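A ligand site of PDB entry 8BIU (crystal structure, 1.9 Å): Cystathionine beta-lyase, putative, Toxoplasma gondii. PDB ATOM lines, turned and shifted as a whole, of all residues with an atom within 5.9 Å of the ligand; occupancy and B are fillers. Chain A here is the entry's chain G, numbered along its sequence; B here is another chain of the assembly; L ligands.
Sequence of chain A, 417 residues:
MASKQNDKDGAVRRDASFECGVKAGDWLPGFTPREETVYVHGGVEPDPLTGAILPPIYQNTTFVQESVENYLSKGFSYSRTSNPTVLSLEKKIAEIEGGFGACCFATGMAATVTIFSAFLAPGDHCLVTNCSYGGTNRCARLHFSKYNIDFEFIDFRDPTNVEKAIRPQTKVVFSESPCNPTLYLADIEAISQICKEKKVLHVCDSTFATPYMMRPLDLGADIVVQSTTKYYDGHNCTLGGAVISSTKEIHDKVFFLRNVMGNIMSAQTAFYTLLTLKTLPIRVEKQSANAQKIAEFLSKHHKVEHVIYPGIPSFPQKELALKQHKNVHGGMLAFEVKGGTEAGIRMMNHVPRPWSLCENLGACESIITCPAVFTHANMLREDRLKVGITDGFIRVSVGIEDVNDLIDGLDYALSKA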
ATOM      1  N   ALA A 106       7.846  -2.254 -17.133  1.00  0.00           N
ATOM      2  CA  ALA A 106       6.403  -2.078 -17.208  1.00  0.00           C
ATOM      3  C   ALA A 106       5.840  -2.653 -18.495  1.00  0.00           C
ATOM      4  O   ALA A 106       4.682  -3.095 -18.515  1.00  0.00           O
ATOM      5  CB  ALA A 106       6.064  -0.586 -17.070  1.00  0.00           C
ATOM      6  N   THR A 107       6.606  -2.640 -19.588  1.00  0.00           N
ATOM      7  CA  THR A 107       6.144  -3.163 -20.872  1.00  0.00           C
ATOM      8  C   THR A 107       7.327  -3.667 -21.674  1.00  0.00           C
ATOM      9  O   THR A 107       8.485  -3.372 -21.376  1.00  0.00           O
ATOM     10  CB  THR A 107       5.445  -2.095 -21.734  1.00  0.00           C
ATOM     11  OG1 THR A 107       6.399  -1.092 -22.069  1.00  0.00           O
ATOM     12  CG2 THR A 107       4.278  -1.466 -21.004  1.00  0.00           C
ATOM     13  N   GLY A 108       7.029  -4.385 -22.753  1.00  0.00           N
ATOM     14  CA  GLY A 108       8.065  -4.727 -23.716  1.00  0.00           C
ATOM     15  C   GLY A 108       8.664  -3.492 -24.360  1.00  0.00           C
ATOM     16  O   GLY A 108       9.877  -3.435 -24.623  1.00  0.00           O
ATOM     17  N   MET A 109       7.837  -2.475 -24.617  1.00  0.00           N
ATOM     18  CA  MET A 109       8.361  -1.273 -25.237  1.00  0.00           C
ATOM     19  C   MET A 109       9.332  -0.563 -24.300  1.00  0.00           C
ATOM     20  O   MET A 109      10.327  -0.007 -24.758  1.00  0.00           O
ATOM     21  CB  MET A 109       7.208  -0.352 -25.637  1.00  0.00           C
ATOM     22  CG  MET A 109       7.562   0.572 -26.746  1.00  0.00           C
ATOM     23  SD  MET A 109       7.773  -0.440 -28.234  1.00  0.00           S
ATOM     24  CE  MET A 109       9.141   0.449 -28.978  1.00  0.00           C
ATOM     25  N   ALA A 110       9.070  -0.574 -22.988  1.00  0.00           N
ATOM     26  CA  ALA A 110      10.019   0.024 -22.065  1.00  0.00           C
ATOM     27  C   ALA A 110      11.346  -0.740 -22.046  1.00  0.00           C
ATOM     28  O   ALA A 110      12.411  -0.130 -21.964  1.00  0.00           O
ATOM     29  CB  ALA A 110       9.420   0.116 -20.661  1.00  0.00           C
ATOM     30  N   THR A 112      12.659  -2.373 -24.594  1.00  0.00           N
ATOM     31  CA  THR A 112      13.331  -1.991 -25.824  1.00  0.00           C
ATOM     32  C   THR A 112      13.941  -0.605 -25.713  1.00  0.00           C
ATOM     33  O   THR A 112      15.086  -0.358 -26.125  1.00  0.00           O
ATOM     34  CB  THR A 112      12.341  -2.013 -26.987  1.00  0.00           C
ATOM     35  OG1 THR A 112      11.693  -3.300 -27.064  1.00  0.00           O
ATOM     36  CG2 THR A 112      13.039  -1.704 -28.299  1.00  0.00           C
ATOM     37  N   TYR A 133       8.800  -5.146 -35.062  1.00  0.00           N
ATOM     38  CA  TYR A 133       7.517  -4.699 -34.527  1.00  0.00           C
ATOM     39  C   TYR A 133       7.357  -3.199 -34.762  1.00  0.00           C
ATOM     40  O   TYR A 133       8.316  -2.430 -34.606  1.00  0.00           O
ATOM     41  CB  TYR A 133       7.435  -5.030 -33.038  1.00  0.00           C
ATOM     42  CG  TYR A 133       6.328  -4.313 -32.305  1.00  0.00           C
ATOM     43  CD1 TYR A 133       5.009  -4.412 -32.735  1.00  0.00           C
ATOM     44  CD2 TYR A 133       6.599  -3.524 -31.182  1.00  0.00           C
ATOM     45  CE1 TYR A 133       3.991  -3.773 -32.066  1.00  0.00           C
ATOM     46  CE2 TYR A 133       5.579  -2.863 -30.515  1.00  0.00           C
ATOM     47  CZ  TYR A 133       4.273  -2.999 -30.960  1.00  0.00           C
ATOM     48  OH  TYR A 133       3.262  -2.352 -30.310  1.00  0.00           O
ATOM     49  N   THR A 136       8.874  -0.699 -32.235  1.00  0.00           N
ATOM     50  CA  THR A 136      10.331  -0.568 -32.226  1.00  0.00           C
ATOM     51  C   THR A 136      10.790   0.396 -33.320  1.00  0.00           C
ATOM     52  O   THR A 136      11.562   1.335 -33.070  1.00  0.00           O
ATOM     53  CB  THR A 136      10.962  -1.946 -32.399  1.00  0.00           C
ATOM     54  OG1 THR A 136      10.392  -2.860 -31.446  1.00  0.00           O
ATOM     55  CG2 THR A 136      12.476  -1.870 -32.196  1.00  0.00           C
ATOM     56  N   GLU A 176      15.061  -9.611 -34.640  1.00  0.00           N
ATOM     57  CA  GLU A 176      13.778 -10.046 -34.106  1.00  0.00           C
ATOM     58  C   GLU A 176      13.384 -11.310 -34.838  1.00  0.00           C
ATOM     59  O   GLU A 176      13.351 -11.309 -36.069  1.00  0.00           O
ATOM     60  CB  GLU A 176      12.721  -8.953 -34.257  1.00  0.00           C
ATOM     61  CG  GLU A 176      11.311  -9.379 -33.932  1.00  0.00           C
ATOM     62  CD  GLU A 176      10.279  -8.289 -34.228  1.00  0.00           C
ATOM     63  OE1 GLU A 176       9.188  -8.605 -34.760  1.00  0.00           O
ATOM     64  OE2 GLU A 176      10.554  -7.111 -33.894  1.00  0.00           O
ATOM     65  N   PRO A 178      10.708 -14.918 -34.587  1.00  0.00           N
ATOM     66  CA  PRO A 178      10.185 -14.495 -35.887  1.00  0.00           C
ATOM     67  C   PRO A 178       9.786 -13.035 -35.863  1.00  0.00           C
ATOM     68  O   PRO A 178       9.567 -12.486 -34.774  1.00  0.00           O
ATOM     69  CB  PRO A 178       8.957 -15.394 -36.097  1.00  0.00           C
ATOM     70  CG  PRO A 178       9.195 -16.571 -35.215  1.00  0.00           C
ATOM     71  CD  PRO A 178       9.923 -16.037 -34.029  1.00  0.00           C
ATOM     72  N   ASN A 180       7.486  -9.613 -36.522  1.00  0.00           N
ATOM     73  CA  ASN A 180       6.100  -9.209 -36.380  1.00  0.00           C
ATOM     74  C   ASN A 180       5.813  -8.150 -37.431  1.00  0.00           C
ATOM     75  O   ASN A 180       6.480  -7.100 -37.438  1.00  0.00           O
ATOM     76  CB  ASN A 180       5.855  -8.666 -34.982  1.00  0.00           C
ATOM     77  CG  ASN A 180       4.478  -8.085 -34.791  1.00  0.00           C
ATOM     78  OD1 ASN A 180       3.636  -8.126 -35.695  1.00  0.00           O
ATOM     79  ND2 ASN A 180       4.218  -7.591 -33.587  1.00  0.00           N
ATOM     80  N   ASP A 205      15.039  -9.665 -30.146  1.00  0.00           N
ATOM     81  CA  ASP A 205      13.664  -9.678 -29.671  1.00  0.00           C
ATOM     82  C   ASP A 205      13.049 -11.003 -30.104  1.00  0.00           C
ATOM     83  O   ASP A 205      12.616 -11.160 -31.250  1.00  0.00           O
ATOM     84  CB  ASP A 205      12.911  -8.491 -30.240  1.00  0.00           C
ATOM     85  CG  ASP A 205      11.523  -8.346 -29.672  1.00  0.00           C
ATOM     86  OD1 ASP A 205      10.950  -9.357 -29.214  1.00  0.00           O
ATOM     87  OD2 ASP A 205      10.993  -7.218 -29.704  1.00  0.00           O
ATOM     88  N   THR A 207      10.298 -12.316 -28.916  1.00  0.00           N
ATOM     89  CA  THR A 207       8.947 -12.352 -28.380  1.00  0.00           C
ATOM     90  C   THR A 207       8.079 -13.385 -29.095  1.00  0.00           C
ATOM     91  O   THR A 207       7.374 -14.161 -28.445  1.00  0.00           O
ATOM     92  CB  THR A 207       8.313 -10.964 -28.496  1.00  0.00           C
ATOM     93  OG1 THR A 207       9.021 -10.039 -27.656  1.00  0.00           O
ATOM     94  CG2 THR A 207       6.864 -11.010 -28.048  1.00  0.00           C
ATOM     95  N   PHE A 208       8.126 -13.414 -30.429  1.00  0.00           N
ATOM     96  CA  PHE A 208       7.285 -14.348 -31.169  1.00  0.00           C
ATOM     97  C   PHE A 208       7.697 -15.804 -30.952  1.00  0.00           C
ATOM     98  O   PHE A 208       6.855 -16.686 -31.099  1.00  0.00           O
ATOM     99  CB  PHE A 208       7.329 -14.036 -32.665  1.00  0.00           C
ATOM    100  CG  PHE A 208       6.273 -13.058 -33.098  1.00  0.00           C
ATOM    101  CD1 PHE A 208       5.972 -11.945 -32.341  1.00  0.00           C
ATOM    102  CD2 PHE A 208       5.602 -13.250 -34.288  1.00  0.00           C
ATOM    103  CE1 PHE A 208       5.014 -11.045 -32.756  1.00  0.00           C
ATOM    104  CE2 PHE A 208       4.638 -12.351 -34.711  1.00  0.00           C
ATOM    105  CZ  PHE A 208       4.340 -11.254 -33.929  1.00  0.00           C
ATOM    106  N   SER A 227       8.665  -8.946 -24.835  1.00  0.00           N
ATOM    107  CA  SER A 227       7.405  -8.426 -24.317  1.00  0.00           C
ATOM    108  C   SER A 227       6.734  -9.579 -23.586  1.00  0.00           C
ATOM    109  O   SER A 227       6.198 -10.490 -24.215  1.00  0.00           O
ATOM    110  CB  SER A 227       6.533  -7.888 -25.444  1.00  0.00           C
ATOM    111  OG  SER A 227       5.229  -7.668 -24.977  1.00  0.00           O
ATOM    112  N   THR A 228       6.803  -9.556 -22.260  1.00  0.00           N
ATOM    113  CA  THR A 228       6.098 -10.576 -21.478  1.00  0.00           C
ATOM    114  C   THR A 228       4.604 -10.438 -21.608  1.00  0.00           C
ATOM    115  O   THR A 228       3.870 -11.368 -21.236  1.00  0.00           O
ATOM    116  CB  THR A 228       6.479 -10.480 -19.993  1.00  0.00           C
ATOM    117  OG1 THR A 228       5.984  -9.254 -19.454  1.00  0.00           O
ATOM    118  CG2 THR A 228       7.972 -10.508 -19.844  1.00  0.00           C
ATOM    119  N   THR A 229       4.122  -9.305 -22.115  1.00  0.00           N
ATOM    120  CA  THR A 229       2.704  -9.149 -22.419  1.00  0.00           C
ATOM    121  C   THR A 229       2.164 -10.343 -23.195  1.00  0.00           C
ATOM    122  O   THR A 229       1.047 -10.810 -22.927  1.00  0.00           O
ATOM    123  CB  THR A 229       2.480  -7.865 -23.232  1.00  0.00           C
ATOM    124  OG1 THR A 229       3.123  -6.751 -22.593  1.00  0.00           O
ATOM    125  CG2 THR A 229       1.003  -7.581 -23.415  1.00  0.00           C
ATOM    126  N   LYS A 230       2.948 -10.842 -24.143  1.00  0.00           N
ATOM    127  CA  LYS A 230       2.433 -11.717 -25.185  1.00  0.00           C
ATOM    128  C   LYS A 230       2.272 -13.176 -24.734  1.00  0.00           C
ATOM    129  O   LYS A 230       1.191 -13.574 -24.317  1.00  0.00           O
ATOM    130  CB  LYS A 230       3.334 -11.640 -26.414  1.00  0.00           C
ATOM    131  CG  LYS A 230       2.912 -10.540 -27.399  1.00  0.00           C
ATOM    132  CD  LYS A 230       3.349  -9.127 -27.015  1.00  0.00           C
ATOM    133  CE  LYS A 230       3.036  -8.137 -28.134  1.00  0.00           C
ATOM    134  NZ  LYS A 230       3.726  -6.829 -27.992  1.00  0.00           N
ATOM    135  N   LEU A 239       0.639  -6.221 -18.867  1.00  0.00           N
ATOM    136  CA  LEU A 239       1.707  -5.710 -19.709  1.00  0.00           C
ATOM    137  C   LEU A 239       3.031  -5.994 -19.012  1.00  0.00           C
ATOM    138  O   LEU A 239       3.114  -6.012 -17.789  1.00  0.00           O
ATOM    139  CB  LEU A 239       1.590  -4.204 -19.977  1.00  0.00           C
ATOM    140  CG  LEU A 239       0.324  -3.647 -20.629  1.00  0.00           C
ATOM    141  CD1 LEU A 239       0.193  -2.148 -20.383  1.00  0.00           C
ATOM    142  CD2 LEU A 239       0.363  -3.946 -22.121  1.00  0.00           C
ATOM    143  N   GLY A 240       4.066  -6.232 -19.805  1.00  0.00           N
ATOM    144  CA  GLY A 240       5.372  -6.414 -19.201  1.00  0.00           C
ATOM    145  C   GLY A 240       6.476  -6.469 -20.217  1.00  0.00           C
ATOM    146  O   GLY A 240       6.225  -6.741 -21.400  1.00  0.00           O
ATOM    147  N   GLY A 241       7.705  -6.188 -19.779  1.00  0.00           N
ATOM    148  CA  GLY A 241       8.876  -6.384 -20.605  1.00  0.00           C
ATOM    149  C   GLY A 241       9.998  -7.020 -19.820  1.00  0.00           C
ATOM    150  O   GLY A 241      10.014  -6.982 -18.596  1.00  0.00           O
ATOM    151  N   LEU A 361      -1.156 -10.630 -28.995  1.00  0.00           N
ATOM    152  CA  LEU A 361      -0.912 -11.934 -29.574  1.00  0.00           C
ATOM    153  C   LEU A 361      -0.364 -12.841 -28.480  1.00  0.00           C
ATOM    154  O   LEU A 361      -0.012 -12.383 -27.392  1.00  0.00           O
ATOM    155  CB  LEU A 361       0.056 -11.831 -30.758  1.00  0.00           C
ATOM    156  CG  LEU A 361       1.438 -11.220 -30.481  1.00  0.00           C
ATOM    157  CD1 LEU A 361       2.498 -12.300 -30.334  1.00  0.00           C
ATOM    158  CD2 LEU A 361       1.830 -10.192 -31.550  1.00  0.00           C
ATOM    159  N   ARG A 395      -2.472 -11.062 -39.923  1.00  0.00           N
ATOM    160  CA  ARG A 395      -1.726 -11.710 -38.858  1.00  0.00           C
ATOM    161  C   ARG A 395      -2.712 -12.402 -37.929  1.00  0.00           C
ATOM    162  O   ARG A 395      -3.752 -11.838 -37.569  1.00  0.00           O
ATOM    163  CB  ARG A 395      -0.896 -10.688 -38.076  1.00  0.00           C
ATOM    164  CG  ARG A 395      -0.095 -11.303 -36.920  1.00  0.00           C
ATOM    165  CD  ARG A 395       0.556 -10.213 -36.082  1.00  0.00           C
ATOM    166  NE  ARG A 395      -0.340  -9.637 -35.064  1.00  0.00           N
ATOM    167  CZ  ARG A 395      -0.016  -8.600 -34.301  1.00  0.00           C
ATOM    168  NH1 ARG A 395       1.167  -8.021 -34.437  1.00  0.00           N
ATOM    169  NH2 ARG A 395      -0.879  -8.132 -33.401  1.00  0.00           N
ATOM    170  N   TYR B  78      -5.298  -0.906 -26.613  1.00  0.00           N
ATOM    171  CA  TYR B  78      -4.117  -1.539 -26.034  1.00  0.00           C
ATOM    172  C   TYR B  78      -3.681  -0.731 -24.810  1.00  0.00           C
ATOM    173  O   TYR B  78      -3.411   0.464 -24.916  1.00  0.00           O
ATOM    174  CB  TYR B  78      -2.991  -1.602 -27.065  1.00  0.00           C
ATOM    175  CG  TYR B  78      -1.869  -2.551 -26.723  1.00  0.00           C
ATOM    176  CD1 TYR B  78      -2.081  -3.912 -26.718  1.00  0.00           C
ATOM    177  CD2 TYR B  78      -0.603  -2.089 -26.460  1.00  0.00           C
ATOM    178  CE1 TYR B  78      -1.058  -4.790 -26.417  1.00  0.00           C
ATOM    179  CE2 TYR B  78       0.434  -2.948 -26.161  1.00  0.00           C
ATOM    180  CZ  TYR B  78       0.193  -4.306 -26.135  1.00  0.00           C
ATOM    181  OH  TYR B  78       1.207  -5.199 -25.838  1.00  0.00           O
ATOM    182  N   ARG B  80      -1.039  -0.403 -23.149  1.00  0.00           N
ATOM    183  CA  ARG B  80       0.191   0.361 -23.116  1.00  0.00           C
ATOM    184  C   ARG B  80      -0.056   1.789 -23.562  1.00  0.00           C
ATOM    185  O   ARG B  80       0.638   2.707 -23.125  1.00  0.00           O
ATOM    186  CB  ARG B  80       1.275  -0.260 -23.988  1.00  0.00           C
ATOM    187  CG  ARG B  80       2.314   0.790 -24.394  1.00  0.00           C
ATOM    188  CD  ARG B  80       3.662   0.242 -24.832  1.00  0.00           C
ATOM    189  NE  ARG B  80       3.539  -0.846 -25.784  1.00  0.00           N
ATOM    190  CZ  ARG B  80       3.102  -0.698 -27.034  1.00  0.00           C
ATOM    191  NH1 ARG B  80       2.744   0.491 -27.491  1.00  0.00           N
ATOM    192  NH2 ARG B  80       3.026  -1.760 -27.823  1.00  0.00           N
ATOM    193  N   GLY B 262       6.515   3.291 -23.378  1.00  0.00           N
ATOM    194  CA  GLY B 262       5.909   2.186 -22.653  1.00  0.00           C
ATOM    195  C   GLY B 262       6.084   2.274 -21.153  1.00  0.00           C
ATOM    196  O   GLY B 262       6.358   1.258 -20.515  1.00  0.00           O
HETATM  197  N1  LIG L   1       8.425  -6.657 -29.662  1.00  0.00           N
HETATM  198  C1  LIG L   1       7.459  -7.351 -30.267  1.00  0.00           C
HETATM  199  C2  LIG L   1       7.822  -8.447 -31.285  1.00  0.00           C
HETATM  200  C3  LIG L   1       6.361  -7.117 -30.017  1.00  0.00           C
HETATM  201  O1  LIG L   1       5.368  -7.851 -30.669  1.00  0.00           O
HETATM  202  C4  LIG L   1       5.923  -6.065 -29.035  1.00  0.00           C
HETATM  203  C5  LIG L   1       4.430  -5.895 -28.809  1.00  0.00           C
HETATM  204  C6  LIG L   1       6.660  -5.417 -28.455  1.00  0.00           C
HETATM  205  C7  LIG L   1       8.039  -5.603 -28.669  1.00  0.00           C
HETATM  206  C8  LIG L   1       6.191  -4.335 -27.468  1.00  0.00           C
HETATM  207  O2  LIG L   1       5.847  -4.902 -26.231  1.00  0.00           O
HETATM  208  P1  LIG L   1       4.671  -4.184 -25.335  1.00  0.00           P
HETATM  209  O3  LIG L   1       4.463  -4.962 -24.060  1.00  0.00           O
HETATM  210  O4  LIG L   1       5.044  -2.777 -24.978  1.00  0.00           O
HETATM  211  O5  LIG L   1       3.394  -4.145 -26.123  1.00  0.00           O
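NZ of Lys 230 is covalently linked to C5 of the ligand (1.4 Å). The side-chain hydroxyl (OH) of Tyr 78 of chain B is in hydrogen-bond range of an oxygen (O5) of the ligand, at 2.4 Å. The guanidinium group (NE) of Arg 80 of chain B is in salt-bridge range of an oxygen (O4) of the ligand (2.6 Å). A nitrogen (N1) of the ligand lies within hydrogen-bond range of the side-chain carboxylate (OD2) of Asp 205 (2.6 Å). O3 of the ligand is in hydrogen-bond range of OG1 of Thr 229 (2.7 Å). The backbone NH (N) of Met 109 is in hydrogen-bond range of an oxygen (O4) of the ligand, 2.8 Å away. The backbone NH (N) of Gly 108 lies within hydrogen-bond range of an oxygen (O3) of the ligand (2.9 Å). The side-chain hydroxyl (OG) of Ser 227 is in hydrogen-bond range of an oxygen (O3) of the ligand, at 3.0 Å. The side-chain amide nitrogen (ND2) of Asn 180 sits at hydrogen-bond distance from an oxygen (O1) of the ligand (3.1 Å).
The side-chain hydroxyl (OG1) of Thr 229 lies close to the side-chain hydroxyl (OG) of Ser 227 (3.3 Å). OG1 of Thr 229 is in hydrogen-bond range of N of Gly 240 (3.0 Å). N of Gly 108 is in hydrogen-bond range of O of Gly 240 (2.8 Å). The backbone carbonyl oxygen of Gly 108 sits at hydrogen-bond distance from the side-chain hydroxyl of Thr 112, 3.0 Å away. OD1 of Asn 180 sits at hydrogen-bond distance from NH1 of Arg 395. N of Ala 110 sits at hydrogen-bond distance from OG1 of Thr 107 (2.9 Å). O of Gly 262 of chain B sits at hydrogen-bond distance from OG1 of Thr 107 (2.8 Å). The backbone carbonyl oxygen of Gly 240 sits at hydrogen-bond distance from the backbone NH of Thr 228 (3.0 Å).
Thr 107 touches the ligand. CD2 of Tyr 133 touches C6 of the ligand (3.3 Å). Glu 176 touches the ligand (OE1 to C2, 3.7 Å). CB of Thr 207 touches C2 of the ligand (3.8 Å). Phe 208 touches the ligand. O of Gly 240 touches O3 of the ligand, at 3.7 Å. Hydrophobic or aromatic side chains within 4 Å of the ligand: Met 109, Tyr 133, Phe 208 and Tyr 78 of chain B. Of the 26 residues printed, 15 come within 4 Å of the ligand. The nearest printed residue that does not touch the ligand is Leu 361 (4.3 Å).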
